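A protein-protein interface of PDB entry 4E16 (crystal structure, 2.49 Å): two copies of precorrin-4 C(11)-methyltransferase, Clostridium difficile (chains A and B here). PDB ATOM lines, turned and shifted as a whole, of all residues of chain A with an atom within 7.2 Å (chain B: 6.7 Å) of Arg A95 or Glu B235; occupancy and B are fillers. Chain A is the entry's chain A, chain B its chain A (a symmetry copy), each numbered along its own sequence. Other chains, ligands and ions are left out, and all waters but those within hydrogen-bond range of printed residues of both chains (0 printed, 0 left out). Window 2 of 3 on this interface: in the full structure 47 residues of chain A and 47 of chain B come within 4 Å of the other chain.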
ATOM      1  N   GLN A  84     -22.079 -17.634 -24.673  1.00  0.00           N
ATOM      2  CA  GLN A  84     -21.370 -18.671 -23.957  1.00  0.00           C
ATOM      3  C   GLN A  84     -21.237 -18.364 -22.482  1.00  0.00           C
ATOM      4  O   GLN A  84     -21.184 -17.212 -22.078  1.00  0.00           O
ATOM      5  CB  GLN A  84     -20.052 -18.984 -24.669  1.00  0.00           C
ATOM      6  CG  GLN A  84     -20.357 -19.622 -26.045  1.00  0.00           C
ATOM      7  CD  GLN A  84     -19.207 -20.390 -26.695  1.00  0.00           C
ATOM      8  OE1 GLN A  84     -19.325 -20.873 -27.838  1.00  0.00           O
ATOM      9  NE2 GLN A  84     -18.089 -20.502 -25.980  1.00  0.00           N
ATOM     10  N   PHE A  88     -15.279 -16.913 -21.915  1.00  0.00           N
ATOM     11  CA  PHE A  88     -14.694 -17.869 -22.849  1.00  0.00           C
ATOM     12  C   PHE A  88     -13.160 -17.836 -22.961  1.00  0.00           C
ATOM     13  O   PHE A  88     -12.559 -18.690 -23.626  1.00  0.00           O
ATOM     14  CB  PHE A  88     -15.330 -17.678 -24.241  1.00  0.00           C
ATOM     15  CG  PHE A  88     -15.702 -16.253 -24.552  1.00  0.00           C
ATOM     16  CD1 PHE A  88     -17.043 -15.859 -24.549  1.00  0.00           C
ATOM     17  CD2 PHE A  88     -14.715 -15.304 -24.833  1.00  0.00           C
ATOM     18  CE1 PHE A  88     -17.389 -14.543 -24.827  1.00  0.00           C
ATOM     19  CE2 PHE A  88     -15.060 -13.991 -25.095  1.00  0.00           C
ATOM     20  CZ  PHE A  88     -16.397 -13.610 -25.098  1.00  0.00           C
ATOM     21  N   GLY A  92     -13.521 -22.018 -22.488  1.00  0.00           N
ATOM     22  CA  GLY A  92     -14.511 -21.465 -23.422  1.00  0.00           C
ATOM     23  C   GLY A  92     -14.614 -22.054 -24.814  1.00  0.00           C
ATOM     24  O   GLY A  92     -15.625 -21.844 -25.491  1.00  0.00           O
ATOM     25  N   SER A  93     -13.583 -22.766 -25.278  1.00  0.00           N
ATOM     26  CA  SER A  93     -13.680 -23.518 -26.552  1.00  0.00           C
ATOM     27  C   SER A  93     -14.206 -22.680 -27.739  1.00  0.00           C
ATOM     28  O   SER A  93     -14.869 -23.199 -28.655  1.00  0.00           O
ATOM     29  CB  SER A  93     -14.584 -24.758 -26.378  1.00  0.00           C
ATOM     30  OG  SER A  93     -14.932 -24.993 -25.014  1.00  0.00           O
ATOM     31  N   ILE A  94     -13.920 -21.385 -27.697  1.00  0.00           N
ATOM     32  CA  ILE A  94     -14.294 -20.436 -28.750  1.00  0.00           C
ATOM     33  C   ILE A  94     -13.378 -20.585 -29.986  1.00  0.00           C
ATOM     34  O   ILE A  94     -13.774 -20.199 -31.081  1.00  0.00           O
ATOM     35  CB  ILE A  94     -14.352 -18.986 -28.149  1.00  0.00           C
ATOM     36  CG1 ILE A  94     -15.684 -18.770 -27.468  1.00  0.00           C
ATOM     37  CG2 ILE A  94     -14.158 -17.841 -29.139  1.00  0.00           C
ATOM     38  CD1 ILE A  94     -16.796 -18.394 -28.417  1.00  0.00           C
ATOM     39  N   ARG A  95     -12.188 -21.183 -29.821  1.00  0.00           N
ATOM     40  CA  ARG A  95     -11.211 -21.306 -30.925  1.00  0.00           C
ATOM     41  C   ARG A  95     -11.779 -22.062 -32.136  1.00  0.00           C
ATOM     42  O   ARG A  95     -11.650 -21.599 -33.263  1.00  0.00           O
ATOM     43  CB  ARG A  95      -9.883 -21.922 -30.453  1.00  0.00           C
ATOM     44  CG  ARG A  95      -8.662 -21.568 -31.302  1.00  0.00           C
ATOM     45  CD  ARG A  95      -7.364 -21.996 -30.624  1.00  0.00           C
ATOM     46  NE  ARG A  95      -7.537 -23.317 -29.987  1.00  0.00           N
ATOM     47  CZ  ARG A  95      -6.650 -24.339 -29.995  1.00  0.00           C
ATOM     48  NH1 ARG A  95      -5.454 -24.260 -30.620  1.00  0.00           N
ATOM     49  NH2 ARG A  95      -6.974 -25.474 -29.368  1.00  0.00           N
ATOM     50  N   GLU A  96     -12.443 -23.190 -31.895  1.00  0.00           N
ATOM     51  CA  GLU A  96     -13.049 -23.964 -32.982  1.00  0.00           C
ATOM     52  C   GLU A  96     -13.923 -23.087 -33.845  1.00  0.00           C
ATOM     53  O   GLU A  96     -13.761 -23.047 -35.074  1.00  0.00           O
ATOM     54  CB  GLU A  96     -13.866 -25.152 -32.464  1.00  0.00           C
ATOM     55  CG  GLU A  96     -13.025 -26.280 -31.884  1.00  0.00           C
ATOM     56  CD  GLU A  96     -13.856 -27.377 -31.230  1.00  0.00           C
ATOM     57  OE1 GLU A  96     -14.794 -27.063 -30.455  1.00  0.00           O
ATOM     58  OE2 GLU A  96     -13.552 -28.564 -31.487  1.00  0.00           O
ATOM     59  N   GLN A  97     -14.843 -22.369 -33.210  1.00  0.00           N
ATOM     60  CA  GLN A  97     -15.806 -21.574 -33.974  1.00  0.00           C
ATOM     61  C   GLN A  97     -15.108 -20.435 -34.726  1.00  0.00           C
ATOM     62  O   GLN A  97     -15.547 -20.065 -35.837  1.00  0.00           O
ATOM     63  CB  GLN A  97     -16.944 -21.066 -33.084  1.00  0.00           C
ATOM     64  CG  GLN A  97     -17.725 -22.188 -32.450  1.00  0.00           C
ATOM     65  CD  GLN A  97     -18.192 -21.832 -31.066  1.00  0.00           C
ATOM     66  OE1 GLN A  97     -19.273 -21.280 -30.918  1.00  0.00           O
ATOM     67  NE2 GLN A  97     -17.366 -22.117 -30.043  1.00  0.00           N
ATOM     68  N   VAL A  98     -14.033 -19.892 -34.134  1.00  0.00           N
ATOM     69  CA  VAL A  98     -13.348 -18.758 -34.767  1.00  0.00           C
ATOM     70  C   VAL A  98     -12.582 -19.194 -35.991  1.00  0.00           C
ATOM     71  O   VAL A  98     -12.813 -18.651 -37.071  1.00  0.00           O
ATOM     72  CB  VAL A  98     -12.463 -17.891 -33.826  1.00  0.00           C
ATOM     73  CG1 VAL A  98     -13.261 -17.450 -32.611  1.00  0.00           C
ATOM     74  CG2 VAL A  98     -11.137 -18.566 -33.444  1.00  0.00           C
ATOM     75  N   GLU A  99     -11.709 -20.187 -35.838  1.00  0.00           N
ATOM     76  CA  GLU A  99     -11.022 -20.730 -36.981  1.00  0.00           C
ATOM     77  C   GLU A  99     -12.013 -21.065 -38.094  1.00  0.00           C
ATOM     78  O   GLU A  99     -11.866 -20.569 -39.209  1.00  0.00           O
ATOM     79  CB  GLU A  99     -10.096 -21.866 -36.582  1.00  0.00           C
ATOM     80  CG  GLU A  99      -8.678 -21.337 -36.361  1.00  0.00           C
ATOM     81  CD  GLU A  99      -8.076 -21.770 -35.032  1.00  0.00           C
ATOM     82  OE1 GLU A  99      -8.327 -22.931 -34.636  1.00  0.00           O
ATOM     83  OE2 GLU A  99      -7.352 -20.961 -34.376  1.00  0.00           O
ATOM     84  N   ASP A 100     -13.075 -21.802 -37.790  1.00  0.00           N
ATOM     85  CA  ASP A 100     -14.075 -22.087 -38.828  1.00  0.00           C
ATOM     86  C   ASP A 100     -14.644 -20.855 -39.535  1.00  0.00           C
ATOM     87  O   ASP A 100     -14.906 -20.912 -40.753  1.00  0.00           O
ATOM     88  CB  ASP A 100     -15.185 -23.035 -38.334  1.00  0.00           C
ATOM     89  CG  ASP A 100     -14.989 -24.479 -38.826  1.00  0.00           C
ATOM     90  OD1 ASP A 100     -14.494 -25.327 -38.039  1.00  0.00           O
ATOM     91  OD2 ASP A 100     -15.306 -24.757 -40.015  1.00  0.00           O
ATOM     92  N   LEU A 101     -14.808 -19.745 -38.809  1.00  0.00           N
ATOM     93  CA  LEU A 101     -15.283 -18.478 -39.419  1.00  0.00           C
ATOM     94  C   LEU A 101     -14.211 -17.746 -40.255  1.00  0.00           C
ATOM     95  O   LEU A 101     -14.530 -17.044 -41.221  1.00  0.00           O
ATOM     96  CB  LEU A 101     -15.878 -17.535 -38.362  1.00  0.00           C
ATOM     97  CG  LEU A 101     -17.130 -18.006 -37.621  1.00  0.00           C
ATOM     98  CD1 LEU A 101     -17.390 -17.216 -36.371  1.00  0.00           C
ATOM     99  CD2 LEU A 101     -18.359 -17.945 -38.500  1.00  0.00           C
ATOM    100  N   ASN A 102     -12.949 -17.887 -39.869  1.00  0.00           N
ATOM    101  CA  ASN A 102     -11.863 -17.368 -40.697  1.00  0.00           C
ATOM    102  C   ASN A 102     -11.900 -18.067 -42.045  1.00  0.00           C
ATOM    103  O   ASN A 102     -12.066 -17.408 -43.075  1.00  0.00           O
ATOM    104  CB  ASN A 102     -10.501 -17.555 -40.027  1.00  0.00           C
ATOM    105  CG  ASN A 102     -10.382 -16.791 -38.709  1.00  0.00           C
ATOM    106  OD1 ASN A 102     -11.055 -15.770 -38.501  1.00  0.00           O
ATOM    107  ND2 ASN A 102      -9.511 -17.280 -37.812  1.00  0.00           N
ATOM    108  N   LEU B 124      -7.747  -8.931 -26.796  1.00  0.00           N
ATOM    109  CA  LEU B 124      -6.771  -9.660 -27.601  1.00  0.00           C
ATOM    110  C   LEU B 124      -7.350 -10.851 -28.401  1.00  0.00           C
ATOM    111  O   LEU B 124      -6.612 -11.497 -29.148  1.00  0.00           O
ATOM    112  CB  LEU B 124      -5.658 -10.179 -26.695  1.00  0.00           C
ATOM    113  CG  LEU B 124      -4.396  -9.354 -26.494  1.00  0.00           C
ATOM    114  CD1 LEU B 124      -3.601 -10.046 -25.415  1.00  0.00           C
ATOM    115  CD2 LEU B 124      -3.577  -9.285 -27.777  1.00  0.00           C
ATOM    116  N   GLY B 125      -8.646 -11.156 -28.244  1.00  0.00           N
ATOM    117  CA  GLY B 125      -9.229 -12.391 -28.818  1.00  0.00           C
ATOM    118  C   GLY B 125      -8.345 -13.611 -28.540  1.00  0.00           C
ATOM    119  O   GLY B 125      -7.721 -14.183 -29.455  1.00  0.00           O
ATOM    120  N   VAL B 126      -8.267 -14.006 -27.268  1.00  0.00           N
ATOM    121  CA  VAL B 126      -7.285 -15.018 -26.860  1.00  0.00           C
ATOM    122  C   VAL B 126      -7.909 -15.708 -25.660  1.00  0.00           C
ATOM    123  O   VAL B 126      -8.832 -15.144 -25.009  1.00  0.00           O
ATOM    124  CB  VAL B 126      -5.904 -14.347 -26.559  1.00  0.00           C
ATOM    125  CG1 VAL B 126      -5.709 -14.023 -25.075  1.00  0.00           C
ATOM    126  CG2 VAL B 126      -4.735 -15.123 -27.136  1.00  0.00           C
ATOM    127  N   GLU B 127      -7.447 -16.928 -25.392  1.00  0.00           N
ATOM    128  CA  GLU B 127      -8.015 -17.773 -24.339  1.00  0.00           C
ATOM    129  C   GLU B 127      -6.899 -18.254 -23.473  1.00  0.00           C
ATOM    130  O   GLU B 127      -5.939 -18.835 -23.981  1.00  0.00           O
ATOM    131  CB  GLU B 127      -8.718 -18.992 -24.937  1.00  0.00           C
ATOM    132  CG  GLU B 127      -9.982 -18.634 -25.705  1.00  0.00           C
ATOM    133  CD  GLU B 127     -10.649 -19.799 -26.446  1.00  0.00           C
ATOM    134  OE1 GLU B 127     -11.574 -19.483 -27.219  1.00  0.00           O
ATOM    135  OE2 GLU B 127     -10.283 -20.991 -26.278  1.00  0.00           O
ATOM    136  N   VAL B 130      -6.095 -23.378 -23.045  1.00  0.00           N
ATOM    137  CA  VAL B 130      -6.174 -23.897 -24.386  1.00  0.00           C
ATOM    138  C   VAL B 130      -5.632 -25.308 -24.355  1.00  0.00           C
ATOM    139  O   VAL B 130      -4.463 -25.502 -23.973  1.00  0.00           O
ATOM    140  CB  VAL B 130      -5.375 -23.016 -25.365  1.00  0.00           C
ATOM    141  CG1 VAL B 130      -5.116 -23.761 -26.683  1.00  0.00           C
ATOM    142  CG2 VAL B 130      -6.125 -21.713 -25.612  1.00  0.00           C
ATOM    143  N   PRO B 131      -6.482 -26.293 -24.748  1.00  0.00           N
ATOM    144  CA  PRO B 131      -6.212 -27.745 -24.710  1.00  0.00           C
ATOM    145  C   PRO B 131      -4.798 -28.142 -25.132  1.00  0.00           C
ATOM    146  O   PRO B 131      -4.341 -27.728 -26.207  1.00  0.00           O
ATOM    147  CB  PRO B 131      -7.233 -28.302 -25.684  1.00  0.00           C
ATOM    148  CG  PRO B 131      -8.399 -27.391 -25.510  1.00  0.00           C
ATOM    149  CD  PRO B 131      -7.840 -26.016 -25.262  1.00  0.00           C
ATOM    150  N   ILE B 133      -2.044 -27.136 -23.976  1.00  0.00           N
ATOM    151  CA  ILE B 133      -1.146 -26.006 -23.754  1.00  0.00           C
ATOM    152  C   ILE B 133      -1.180 -25.511 -22.269  1.00  0.00           C
ATOM    153  O   ILE B 133      -0.152 -25.531 -21.561  1.00  0.00           O
ATOM    154  CB  ILE B 133      -1.414 -24.934 -24.847  1.00  0.00           C
ATOM    155  CG1 ILE B 133      -1.027 -25.513 -26.222  1.00  0.00           C
ATOM    156  CG2 ILE B 133      -0.664 -23.642 -24.559  1.00  0.00           C
ATOM    157  CD1 ILE B 133      -1.665 -24.842 -27.425  1.00  0.00           C
ATOM    158  N   PRO B 190       5.795 -16.215 -25.991  1.00  0.00           N
ATOM    159  CA  PRO B 190       5.087 -14.981 -26.299  1.00  0.00           C
ATOM    160  C   PRO B 190       4.657 -14.250 -25.035  1.00  0.00           C
ATOM    161  O   PRO B 190       4.310 -14.884 -24.011  1.00  0.00           O
ATOM    162  CB  PRO B 190       3.841 -15.463 -27.051  1.00  0.00           C
ATOM    163  CG  PRO B 190       4.109 -16.885 -27.402  1.00  0.00           C
ATOM    164  CD  PRO B 190       5.005 -17.409 -26.337  1.00  0.00           C
ATOM    165  N   LYS B 206       2.814  -6.448 -28.211  1.00  0.00           N
ATOM    166  CA  LYS B 206       3.007  -7.868 -28.400  1.00  0.00           C
ATOM    167  C   LYS B 206       4.476  -8.192 -28.626  1.00  0.00           C
ATOM    168  O   LYS B 206       5.181  -7.439 -29.288  1.00  0.00           O
ATOM    169  CB  LYS B 206       2.230  -8.273 -29.638  1.00  0.00           C
ATOM    170  CG  LYS B 206       0.846  -8.811 -29.357  1.00  0.00           C
ATOM    171  CD  LYS B 206       0.775 -10.301 -29.711  1.00  0.00           C
ATOM    172  CE  LYS B 206       1.430 -11.244 -28.688  1.00  0.00           C
ATOM    173  NZ  LYS B 206       0.921 -12.634 -28.923  1.00  0.00           N
ATOM    174  N   ARG B 231       2.294 -19.697 -23.732  1.00  0.00           N
ATOM    175  CA  ARG B 231       2.161 -20.261 -25.077  1.00  0.00           C
ATOM    176  C   ARG B 231       0.785 -19.937 -25.616  1.00  0.00           C
ATOM    177  O   ARG B 231       0.585 -19.915 -26.808  1.00  0.00           O
ATOM    178  CB  ARG B 231       2.502 -21.779 -25.099  1.00  0.00           C
ATOM    179  CG  ARG B 231       4.012 -22.081 -25.140  1.00  0.00           C
ATOM    180  CD  ARG B 231       4.643 -21.070 -26.108  1.00  0.00           C
ATOM    181  NE  ARG B 231       6.015 -21.305 -26.591  1.00  0.00           N
ATOM    182  CZ  ARG B 231       6.448 -20.944 -27.809  1.00  0.00           C
ATOM    183  NH1 ARG B 231       5.624 -20.361 -28.689  1.00  0.00           N
ATOM    184  NH2 ARG B 231       7.705 -21.186 -28.166  1.00  0.00           N
ATOM    185  N   PHE B 232      -0.137 -19.602 -24.717  1.00  0.00           N
ATOM    186  CA  PHE B 232      -1.541 -19.376 -25.073  1.00  0.00           C
ATOM    187  C   PHE B 232      -1.727 -18.151 -25.943  1.00  0.00           C
ATOM    188  O   PHE B 232      -2.800 -17.960 -26.545  1.00  0.00           O
ATOM    189  CB  PHE B 232      -2.397 -19.285 -23.799  1.00  0.00           C
ATOM    190  CG  PHE B 232      -2.335 -17.938 -23.112  1.00  0.00           C
ATOM    191  CD1 PHE B 232      -3.217 -16.923 -23.458  1.00  0.00           C
ATOM    192  CD2 PHE B 232      -1.384 -17.691 -22.125  1.00  0.00           C
ATOM    193  CE1 PHE B 232      -3.134 -15.674 -22.835  1.00  0.00           C
ATOM    194  CE2 PHE B 232      -1.294 -16.454 -21.509  1.00  0.00           C
ATOM    195  CZ  PHE B 232      -2.167 -15.442 -21.857  1.00  0.00           C
ATOM    196  N   LEU B 233      -0.700 -17.298 -25.977  1.00  0.00           N
ATOM    197  CA  LEU B 233      -0.648 -16.155 -26.908  1.00  0.00           C
ATOM    198  C   LEU B 233      -0.245 -16.567 -28.330  1.00  0.00           C
ATOM    199  O   LEU B 233      -0.507 -15.839 -29.277  1.00  0.00           O
ATOM    200  CB  LEU B 233       0.338 -15.097 -26.425  1.00  0.00           C
ATOM    201  CG  LEU B 233       0.073 -14.136 -25.275  1.00  0.00           C
ATOM    202  CD1 LEU B 233      -1.414 -13.943 -25.072  1.00  0.00           C
ATOM    203  CD2 LEU B 233       0.769 -14.613 -24.004  1.00  0.00           C
ATOM    204  N   GLY B 234       0.415 -17.722 -28.466  1.00  0.00           N
ATOM    205  CA  GLY B 234       0.712 -18.322 -29.767  1.00  0.00           C
ATOM    206  C   GLY B 234      -0.520 -18.651 -30.606  1.00  0.00           C
ATOM    207  O   GLY B 234      -0.349 -19.000 -31.786  1.00  0.00           O
ATOM    208  N   GLU B 235      -1.736 -18.550 -30.001  1.00  0.00           N
ATOM    209  CA  GLU B 235      -3.109 -18.771 -30.633  1.00  0.00           C
ATOM    210  C   GLU B 235      -4.072 -17.540 -30.552  1.00  0.00           C
ATOM    211  O   GLU B 235      -4.650 -17.075 -31.546  1.00  0.00           O
ATOM    212  CB  GLU B 235      -3.833 -20.007 -30.020  1.00  0.00           C
ATOM    213  CG  GLU B 235      -2.939 -21.177 -29.533  1.00  0.00           C
ATOM    214  CD  GLU B 235      -2.641 -22.305 -30.576  1.00  0.00           C
ATOM    215  OE1 GLU B 235      -3.402 -22.494 -31.576  1.00  0.00           O
ATOM    216  OE2 GLU B 235      -1.633 -23.043 -30.381  1.00  0.00           O
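Of the printed residues of chain B, Ser A93 touches Glu B127.
Arg A95 touches just these residues of chain B: Glu B127, Val B130 and Glu B235.
Asp A100 touches none of the printed residues of chain B.
Leu A101 touches none of the printed residues of chain B.
Of the printed residues of chain A, Glu B127 touches Phe A88, Ser A93, Ile A94 and Arg A95.
Printed residues of chain A within 4 Å of Val B130: Arg A95 (3.7 Å).
No residue of chain A comes within 4 Å of Gly B234.
Of chain A, only Arg A95 comes within 4 Å of Glu B235.
The nearest residue of chain B that does not touch Arg A95 is Pro B131 (4.2 Å).
The backbone carbonyl oxygen (O) of Ser A93 sits at hydrogen-bond distance from the side-chain amide nitrogen (NE2) of Gln A97.
Of the 14 printed residues of chain B, 3 touch a printed residue of chain A.
Hydrophobic or aromatic side chains of chain A that line the printed part of chain B: Ile A94.
Along chain A the printed residues that touch a printed residue of chain B span positions 88 to 95.
Among the printed residues, Asp or Glu carboxylates within 4 Å of a Lys or Arg side-chain nitrogen of the other chain: Arg A95 with Glu B235 (2.9 Å).
N of Ile A94 sits close to OE1 of Glu B127, 3.1 Å away.
OE1 of Glu B127 is in hydrogen-bond range of N of Arg A95, 3.2 Å away.
The guanidinium group of Arg A95 is in salt-bridge range of the side-chain carboxylate of Glu B235 (2.9 Å).
No position is printed for both chains.
Phe A88 touches Glu B127.
OE2 of Glu B127 touches N of Ser A93 (3.9 Å).
NH2 of Arg A95 touches CG1 of Val B130, at 3.7 Å.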
